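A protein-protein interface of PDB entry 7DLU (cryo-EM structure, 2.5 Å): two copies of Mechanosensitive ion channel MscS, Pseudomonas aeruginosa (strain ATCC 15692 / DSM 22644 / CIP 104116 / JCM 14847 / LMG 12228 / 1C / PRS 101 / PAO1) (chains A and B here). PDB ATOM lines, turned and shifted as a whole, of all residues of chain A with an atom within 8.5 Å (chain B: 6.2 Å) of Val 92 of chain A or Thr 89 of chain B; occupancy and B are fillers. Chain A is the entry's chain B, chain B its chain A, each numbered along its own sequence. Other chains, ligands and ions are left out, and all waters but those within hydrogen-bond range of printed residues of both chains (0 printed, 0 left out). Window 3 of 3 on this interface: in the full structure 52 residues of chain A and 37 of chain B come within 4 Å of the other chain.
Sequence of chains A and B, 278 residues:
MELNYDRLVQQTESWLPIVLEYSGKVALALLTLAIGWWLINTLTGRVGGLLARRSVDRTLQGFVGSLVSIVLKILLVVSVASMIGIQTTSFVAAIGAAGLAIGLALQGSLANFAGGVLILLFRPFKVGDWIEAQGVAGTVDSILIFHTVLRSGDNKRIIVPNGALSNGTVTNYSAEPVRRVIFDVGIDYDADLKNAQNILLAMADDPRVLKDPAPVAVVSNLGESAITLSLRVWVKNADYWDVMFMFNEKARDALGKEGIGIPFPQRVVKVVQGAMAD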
ATOM      1  N   ILE A  74      19.883 -17.696   7.470  1.00  0.00           N
ATOM      2  CA  ILE A  74      21.273 -17.271   7.335  1.00  0.00           C
ATOM      3  C   ILE A  74      21.714 -16.502   8.573  1.00  0.00           C
ATOM      4  O   ILE A  74      22.794 -16.746   9.126  1.00  0.00           O
ATOM      5  CB  ILE A  74      21.458 -16.435   6.056  1.00  0.00           C
ATOM      6  CG1 ILE A  74      21.431 -17.330   4.821  1.00  0.00           C
ATOM      7  CG2 ILE A  74      22.758 -15.661   6.106  1.00  0.00           C
ATOM      8  CD1 ILE A  74      21.535 -16.568   3.525  1.00  0.00           C
ATOM      9  N   LEU A  75      20.883 -15.559   9.027  1.00  0.00           N
ATOM     10  CA  LEU A  75      21.235 -14.789  10.219  1.00  0.00           C
ATOM     11  C   LEU A  75      21.426 -15.699  11.430  1.00  0.00           C
ATOM     12  O   LEU A  75      22.418 -15.583  12.161  1.00  0.00           O
ATOM     13  CB  LEU A  75      20.168 -13.734  10.498  1.00  0.00           C
ATOM     14  CG  LEU A  75      20.006 -12.619   9.466  1.00  0.00           C
ATOM     15  CD1 LEU A  75      18.919 -11.657   9.893  1.00  0.00           C
ATOM     16  CD2 LEU A  75      21.310 -11.883   9.248  1.00  0.00           C
ATOM     17  N   VAL A  78      24.667 -17.901  11.126  1.00  0.00           N
ATOM     18  CA  VAL A  78      25.857 -17.101  11.408  1.00  0.00           C
ATOM     19  C   VAL A  78      25.989 -16.854  12.906  1.00  0.00           C
ATOM     20  O   VAL A  78      27.081 -16.978  13.481  1.00  0.00           O
ATOM     21  CB  VAL A  78      25.817 -15.782  10.615  1.00  0.00           C
ATOM     22  CG1 VAL A  78      26.887 -14.830  11.107  1.00  0.00           C
ATOM     23  CG2 VAL A  78      25.998 -16.051   9.137  1.00  0.00           C
ATOM     24  N   SER A  79      24.875 -16.536  13.570  1.00  0.00           N
ATOM     25  CA  SER A  79      24.925 -16.250  15.001  1.00  0.00           C
ATOM     26  C   SER A  79      25.389 -17.466  15.799  1.00  0.00           C
ATOM     27  O   SER A  79      26.264 -17.355  16.663  1.00  0.00           O
ATOM     28  CB  SER A  79      23.559 -15.771  15.488  1.00  0.00           C
ATOM     29  OG  SER A  79      23.323 -16.173  16.824  1.00  0.00           O
ATOM     30  N   SER A  82      29.079 -18.368  15.212  1.00  0.00           N
ATOM     31  CA  SER A  82      29.948 -17.514  16.012  1.00  0.00           C
ATOM     32  C   SER A  82      29.818 -17.827  17.496  1.00  0.00           C
ATOM     33  O   SER A  82      30.754 -17.582  18.263  1.00  0.00           O
ATOM     34  CB  SER A  82      29.629 -16.045  15.753  1.00  0.00           C
ATOM     35  OG  SER A  82      29.840 -15.273  16.918  1.00  0.00           O
ATOM     36  N   GLN A  87      35.069 -17.723  13.998  1.00  0.00           N
ATOM     37  CA  GLN A  87      35.139 -16.307  13.662  1.00  0.00           C
ATOM     38  C   GLN A  87      34.330 -16.047  12.399  1.00  0.00           C
ATOM     39  O   GLN A  87      34.576 -16.667  11.360  1.00  0.00           O
ATOM     40  CB  GLN A  87      36.591 -15.881  13.466  1.00  0.00           C
ATOM     41  CG  GLN A  87      37.472 -16.108  14.674  1.00  0.00           C
ATOM     42  CD  GLN A  87      37.569 -14.883  15.554  1.00  0.00           C
ATOM     43  OE1 GLN A  87      37.888 -14.980  16.736  1.00  0.00           O
ATOM     44  NE2 GLN A  87      37.292 -13.720  14.980  1.00  0.00           N
ATOM     45  N   THR A  88      33.367 -15.130  12.482  1.00  0.00           N
ATOM     46  CA  THR A  88      32.450 -14.878  11.378  1.00  0.00           C
ATOM     47  C   THR A  88      32.400 -13.402  11.005  1.00  0.00           C
ATOM     48  O   THR A  88      31.361 -12.906  10.577  1.00  0.00           O
ATOM     49  CB  THR A  88      31.044 -15.382  11.710  1.00  0.00           C
ATOM     50  OG1 THR A  88      30.591 -14.777  12.926  1.00  0.00           O
ATOM     51  CG2 THR A  88      31.036 -16.891  11.869  1.00  0.00           C
ATOM     52  N   THR A  89      33.513 -12.684  11.153  1.00  0.00           N
ATOM     53  CA  THR A  89      33.515 -11.268  10.799  1.00  0.00           C
ATOM     54  C   THR A  89      33.373 -11.075   9.293  1.00  0.00           C
ATOM     55  O   THR A  89      32.716 -10.127   8.843  1.00  0.00           O
ATOM     56  CB  THR A  89      34.790 -10.599  11.313  1.00  0.00           C
ATOM     57  OG1 THR A  89      35.042 -11.017  12.658  1.00  0.00           O
ATOM     58  CG2 THR A  89      34.643  -9.095  11.300  1.00  0.00           C
ATOM     59  N   SER A  90      33.963 -11.974   8.500  1.00  0.00           N
ATOM     60  CA  SER A  90      33.842 -11.887   7.047  1.00  0.00           C
ATOM     61  C   SER A  90      32.405 -12.100   6.596  1.00  0.00           C
ATOM     62  O   SER A  90      31.912 -11.402   5.701  1.00  0.00           O
ATOM     63  CB  SER A  90      34.757 -12.915   6.389  1.00  0.00           C
ATOM     64  OG  SER A  90      36.104 -12.702   6.753  1.00  0.00           O
ATOM     65  N   PHE A  91      31.716 -13.061   7.203  1.00  0.00           N
ATOM     66  CA  PHE A  91      30.331 -13.313   6.843  1.00  0.00           C
ATOM     67  C   PHE A  91      29.413 -12.191   7.304  1.00  0.00           C
ATOM     68  O   PHE A  91      28.436 -11.883   6.620  1.00  0.00           O
ATOM     69  CB  PHE A  91      29.887 -14.657   7.414  1.00  0.00           C
ATOM     70  CG  PHE A  91      30.681 -15.814   6.894  1.00  0.00           C
ATOM     71  CD1 PHE A  91      30.361 -16.400   5.684  1.00  0.00           C
ATOM     72  CD2 PHE A  91      31.762 -16.304   7.603  1.00  0.00           C
ATOM     73  CE1 PHE A  91      31.094 -17.459   5.197  1.00  0.00           C
ATOM     74  CE2 PHE A  91      32.501 -17.363   7.119  1.00  0.00           C
ATOM     75  CZ  PHE A  91      32.166 -17.940   5.916  1.00  0.00           C
ATOM     76  N   VAL A  92      29.720 -11.554   8.432  1.00  0.00           N
ATOM     77  CA  VAL A  92      28.932 -10.403   8.855  1.00  0.00           C
ATOM     78  C   VAL A  92      29.144  -9.235   7.898  1.00  0.00           C
ATOM     79  O   VAL A  92      28.198  -8.517   7.557  1.00  0.00           O
ATOM     80  CB  VAL A  92      29.273 -10.027  10.308  1.00  0.00           C
ATOM     81  CG1 VAL A  92      28.660  -8.689  10.672  1.00  0.00           C
ATOM     82  CG2 VAL A  92      28.779 -11.102  11.255  1.00  0.00           C
ATOM     83  N   ALA A  93      30.378  -9.041   7.430  1.00  0.00           N
ATOM     84  CA  ALA A  93      30.635  -8.006   6.433  1.00  0.00           C
ATOM     85  C   ALA A  93      29.883  -8.285   5.136  1.00  0.00           C
ATOM     86  O   ALA A  93      29.308  -7.372   4.531  1.00  0.00           O
ATOM     87  CB  ALA A  93      32.135  -7.893   6.171  1.00  0.00           C
ATOM     88  N   ALA A  94      29.873  -9.545   4.696  1.00  0.00           N
ATOM     89  CA  ALA A  94      29.145  -9.899   3.481  1.00  0.00           C
ATOM     90  C   ALA A  94      27.644  -9.694   3.652  1.00  0.00           C
ATOM     91  O   ALA A  94      26.964  -9.215   2.737  1.00  0.00           O
ATOM     92  CB  ALA A  94      29.447 -11.345   3.094  1.00  0.00           C
ATOM     93  N   ILE A  95      27.108 -10.057   4.819  1.00  0.00           N
ATOM     94  CA  ILE A  95      25.687  -9.861   5.088  1.00  0.00           C
ATOM     95  C   ILE A  95      25.347  -8.378   5.083  1.00  0.00           C
ATOM     96  O   ILE A  95      24.307  -7.969   4.559  1.00  0.00           O
ATOM     97  CB  ILE A  95      25.298 -10.536   6.417  1.00  0.00           C
ATOM     98  CG1 ILE A  95      24.669 -11.907   6.160  1.00  0.00           C
ATOM     99  CG2 ILE A  95      24.339  -9.667   7.222  1.00  0.00           C
ATOM    100  CD1 ILE A  95      25.550 -12.853   5.379  1.00  0.00           C
ATOM    101  N   GLY A  96      26.220  -7.550   5.656  1.00  0.00           N
ATOM    102  CA  GLY A  96      25.983  -6.118   5.638  1.00  0.00           C
ATOM    103  C   GLY A  96      26.008  -5.542   4.236  1.00  0.00           C
ATOM    104  O   GLY A  96      25.187  -4.690   3.889  1.00  0.00           O
ATOM    105  N   ALA A  97      26.945  -6.007   3.407  1.00  0.00           N
ATOM    106  CA  ALA A  97      26.996  -5.552   2.021  1.00  0.00           C
ATOM    107  C   ALA A  97      25.731  -5.945   1.262  1.00  0.00           C
ATOM    108  O   ALA A  97      25.160  -5.135   0.521  1.00  0.00           O
ATOM    109  CB  ALA A  97      28.234  -6.116   1.329  1.00  0.00           C
ATOM    110  N   ALA A  98      25.276  -7.187   1.440  1.00  0.00           N
ATOM    111  CA  ALA A  98      24.059  -7.628   0.762  1.00  0.00           C
ATOM    112  C   ALA A  98      22.838  -6.861   1.253  1.00  0.00           C
ATOM    113  O   ALA A  98      21.954  -6.515   0.460  1.00  0.00           O
ATOM    114  CB  ALA A  98      23.863  -9.130   0.954  1.00  0.00           C
ATOM    115  N   GLY A  99      22.769  -6.584   2.555  1.00  0.00           N
ATOM    116  CA  GLY A  99      21.657  -5.810   3.078  1.00  0.00           C
ATOM    117  C   GLY A  99      21.643  -4.387   2.560  1.00  0.00           C
ATOM    118  O   GLY A  99      20.585  -3.842   2.247  1.00  0.00           O
ATOM    119  N   GLN B  87      24.929 -14.263  20.577  1.00  0.00           N
ATOM    120  CA  GLN B  87      25.633 -13.377  19.660  1.00  0.00           C
ATOM    121  C   GLN B  87      24.649 -12.829  18.634  1.00  0.00           C
ATOM    122  O   GLN B  87      23.980 -13.597  17.938  1.00  0.00           O
ATOM    123  CB  GLN B  87      26.768 -14.124  18.967  1.00  0.00           C
ATOM    124  CG  GLN B  87      27.794 -14.708  19.913  1.00  0.00           C
ATOM    125  CD  GLN B  87      28.968 -13.782  20.132  1.00  0.00           C
ATOM    126  OE1 GLN B  87      29.675 -13.886  21.130  1.00  0.00           O
ATOM    127  NE2 GLN B  87      29.181 -12.867  19.196  1.00  0.00           N
ATOM    128  N   THR B  88      24.561 -11.502  18.537  1.00  0.00           N
ATOM    129  CA  THR B  88      23.574 -10.860  17.679  1.00  0.00           C
ATOM    130  C   THR B  88      24.213  -9.855  16.730  1.00  0.00           C
ATOM    131  O   THR B  88      23.595  -8.849  16.386  1.00  0.00           O
ATOM    132  CB  THR B  88      22.488 -10.177  18.512  1.00  0.00           C
ATOM    133  OG1 THR B  88      23.091  -9.247  19.419  1.00  0.00           O
ATOM    134  CG2 THR B  88      21.692 -11.201  19.301  1.00  0.00           C
ATOM    135  N   THR B  89      25.446 -10.107  16.291  1.00  0.00           N
ATOM    136  CA  THR B  89      26.094  -9.176  15.373  1.00  0.00           C
ATOM    137  C   THR B  89      25.411  -9.179  14.010  1.00  0.00           C
ATOM    138  O   THR B  89      25.302  -8.130  13.362  1.00  0.00           O
ATOM    139  CB  THR B  89      27.577  -9.519  15.237  1.00  0.00           C
ATOM    140  OG1 THR B  89      28.131  -9.774  16.532  1.00  0.00           O
ATOM    141  CG2 THR B  89      28.333  -8.368  14.614  1.00  0.00           C
ATOM    142  N   SER B  90      24.929 -10.343  13.567  1.00  0.00           N
ATOM    143  CA  SER B  90      24.225 -10.427  12.291  1.00  0.00           C
ATOM    144  C   SER B  90      22.922  -9.643  12.323  1.00  0.00           C
ATOM    145  O   SER B  90      22.573  -8.953  11.357  1.00  0.00           O
ATOM    146  CB  SER B  90      23.950 -11.887  11.946  1.00  0.00           C
ATOM    147  OG  SER B  90      25.152 -12.623  11.857  1.00  0.00           O
ATOM    148  N   PHE B  91      22.186  -9.737  13.426  1.00  0.00           N
ATOM    149  CA  PHE B  91      20.938  -9.003  13.543  1.00  0.00           C
ATOM    150  C   PHE B  91      21.172  -7.506  13.676  1.00  0.00           C
ATOM    151  O   PHE B  91      20.371  -6.716  13.175  1.00  0.00           O
ATOM    152  CB  PHE B  91      20.132  -9.540  14.723  1.00  0.00           C
ATOM    153  CG  PHE B  91      19.765 -10.985  14.581  1.00  0.00           C
ATOM    154  CD1 PHE B  91      18.654 -11.360  13.853  1.00  0.00           C
ATOM    155  CD2 PHE B  91      20.545 -11.971  15.159  1.00  0.00           C
ATOM    156  CE1 PHE B  91      18.318 -12.688  13.712  1.00  0.00           C
ATOM    157  CE2 PHE B  91      20.214 -13.302  15.020  1.00  0.00           C
ATOM    158  CZ  PHE B  91      19.100 -13.660  14.297  1.00  0.00           C
ATOM    159  N   VAL B  92      22.267  -7.098  14.315  1.00  0.00           N
ATOM    160  CA  VAL B  92      22.589  -5.677  14.373  1.00  0.00           C
ATOM    161  C   VAL B  92      22.958  -5.161  12.987  1.00  0.00           C
ATOM    162  O   VAL B  92      22.572  -4.053  12.601  1.00  0.00           O
ATOM    163  CB  VAL B  92      23.708  -5.424  15.399  1.00  0.00           C
ATOM    164  CG1 VAL B  92      24.227  -4.004  15.284  1.00  0.00           C
ATOM    165  CG2 VAL B  92      23.196  -5.680  16.802  1.00  0.00           C
ATOM    166  N   ALA B  93      23.687  -5.961  12.208  1.00  0.00           N
ATOM    167  CA  ALA B  93      23.992  -5.575  10.833  1.00  0.00           C
ATOM    168  C   ALA B  93      22.724  -5.449   9.997  1.00  0.00           C
ATOM    169  O   ALA B  93      22.578  -4.505   9.210  1.00  0.00           O
ATOM    170  CB  ALA B  93      24.952  -6.585  10.207  1.00  0.00           C
ATOM    171  N   ALA B  94      21.791  -6.390  10.157  1.00  0.00           N
ATOM    172  CA  ALA B  94      20.534  -6.320   9.419  1.00  0.00           C
ATOM    173  C   ALA B  94      19.715  -5.102   9.830  1.00  0.00           C
ATOM    174  O   ALA B  94      19.106  -4.437   8.983  1.00  0.00           O
ATOM    175  CB  ALA B  94      19.732  -7.602   9.632  1.00  0.00           C
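Of chain B, only Thr 89 (3.97 Å) and Ser 90 (3.98 Å) come within 4 Å of Val 92 of chain A.
Thr 89 of chain B touches one residue of chain A.
Ser 90 of chain B touches three residues of chain A.
Of the printed residues of chain B, Ser 79 of chain A touches Gln 87.
Of the printed residues of chain A, Gln 87 of chain B touches Ser 79 and Ser 82.
Printed residues of chain B within 4 Å of Leu 75 of chain A: Ser 90 (3.8 Å) and Phe 91 (3.9 Å).
Of the printed residues of chain B, Val 78 of chain A touches Ser 90.
Ala 98 of chain A touches none of the printed residues of chain B.
The nearest residue of chain B that does not touch Val 92 of chain A is Ala 93 of chain B (4.3 Å).
The nearest residue of chain A that does not touch Thr 89 of chain B is Ser 82 of chain A (5.8 Å).
The nearest printed residue of chain B that does not touch Ser 79 of chain A is Phe 91 of chain B (4.2 Å).
Printed residues of chain A that touch a printed residue of chain B: Leu 75, Val 78, Ser 79, Ser 82 and Val 92.
Among the printed residues, 7 pairs touch across the chains.
Among the printed residues, no Asp or Glu carboxylate lies within 4 Å of a Lys or Arg side-chain nitrogen of the other chain.
Val 92 of chain A touches Thr 89 of chain B, but with the chains exchanged Thr 89 of chain A does not touch Val 92 of chain B (11.7 Å).
Val 92 of chain A touches Ser 90 of chain B, but with the chains exchanged Ser 90 of chain A does not touch Val 92 of chain B (13.1 Å).
Positions printed for both chains: 87, 88, 89, 90, 91, 92, 93 and 94.
Of the 7 pairs that touch across the chains among the printed residues, none has its exchanged pair printed and touching as well.
Among the printed residues, pairs that only touch across the chains: Val 78 of chain A with Ser 90 of chain B, Leu 75 of chain A with Ser 90 of chain B, Leu 75 of chain A with Phe 91 of chain B, Val 92 of chain A with Thr 89 of chain B and Val 92 of chain A with Ser 90 of chain B.
The backbone carbonyl oxygen (O) of Gln 87 of chain B is in hydrogen-bond range of the side-chain hydroxyl (OG) of Ser 79 of chain A.
OG of Ser 82 of chain A lies within hydrogen-bond range of NE2 of Gln 87 of chain B (3.4 Å).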
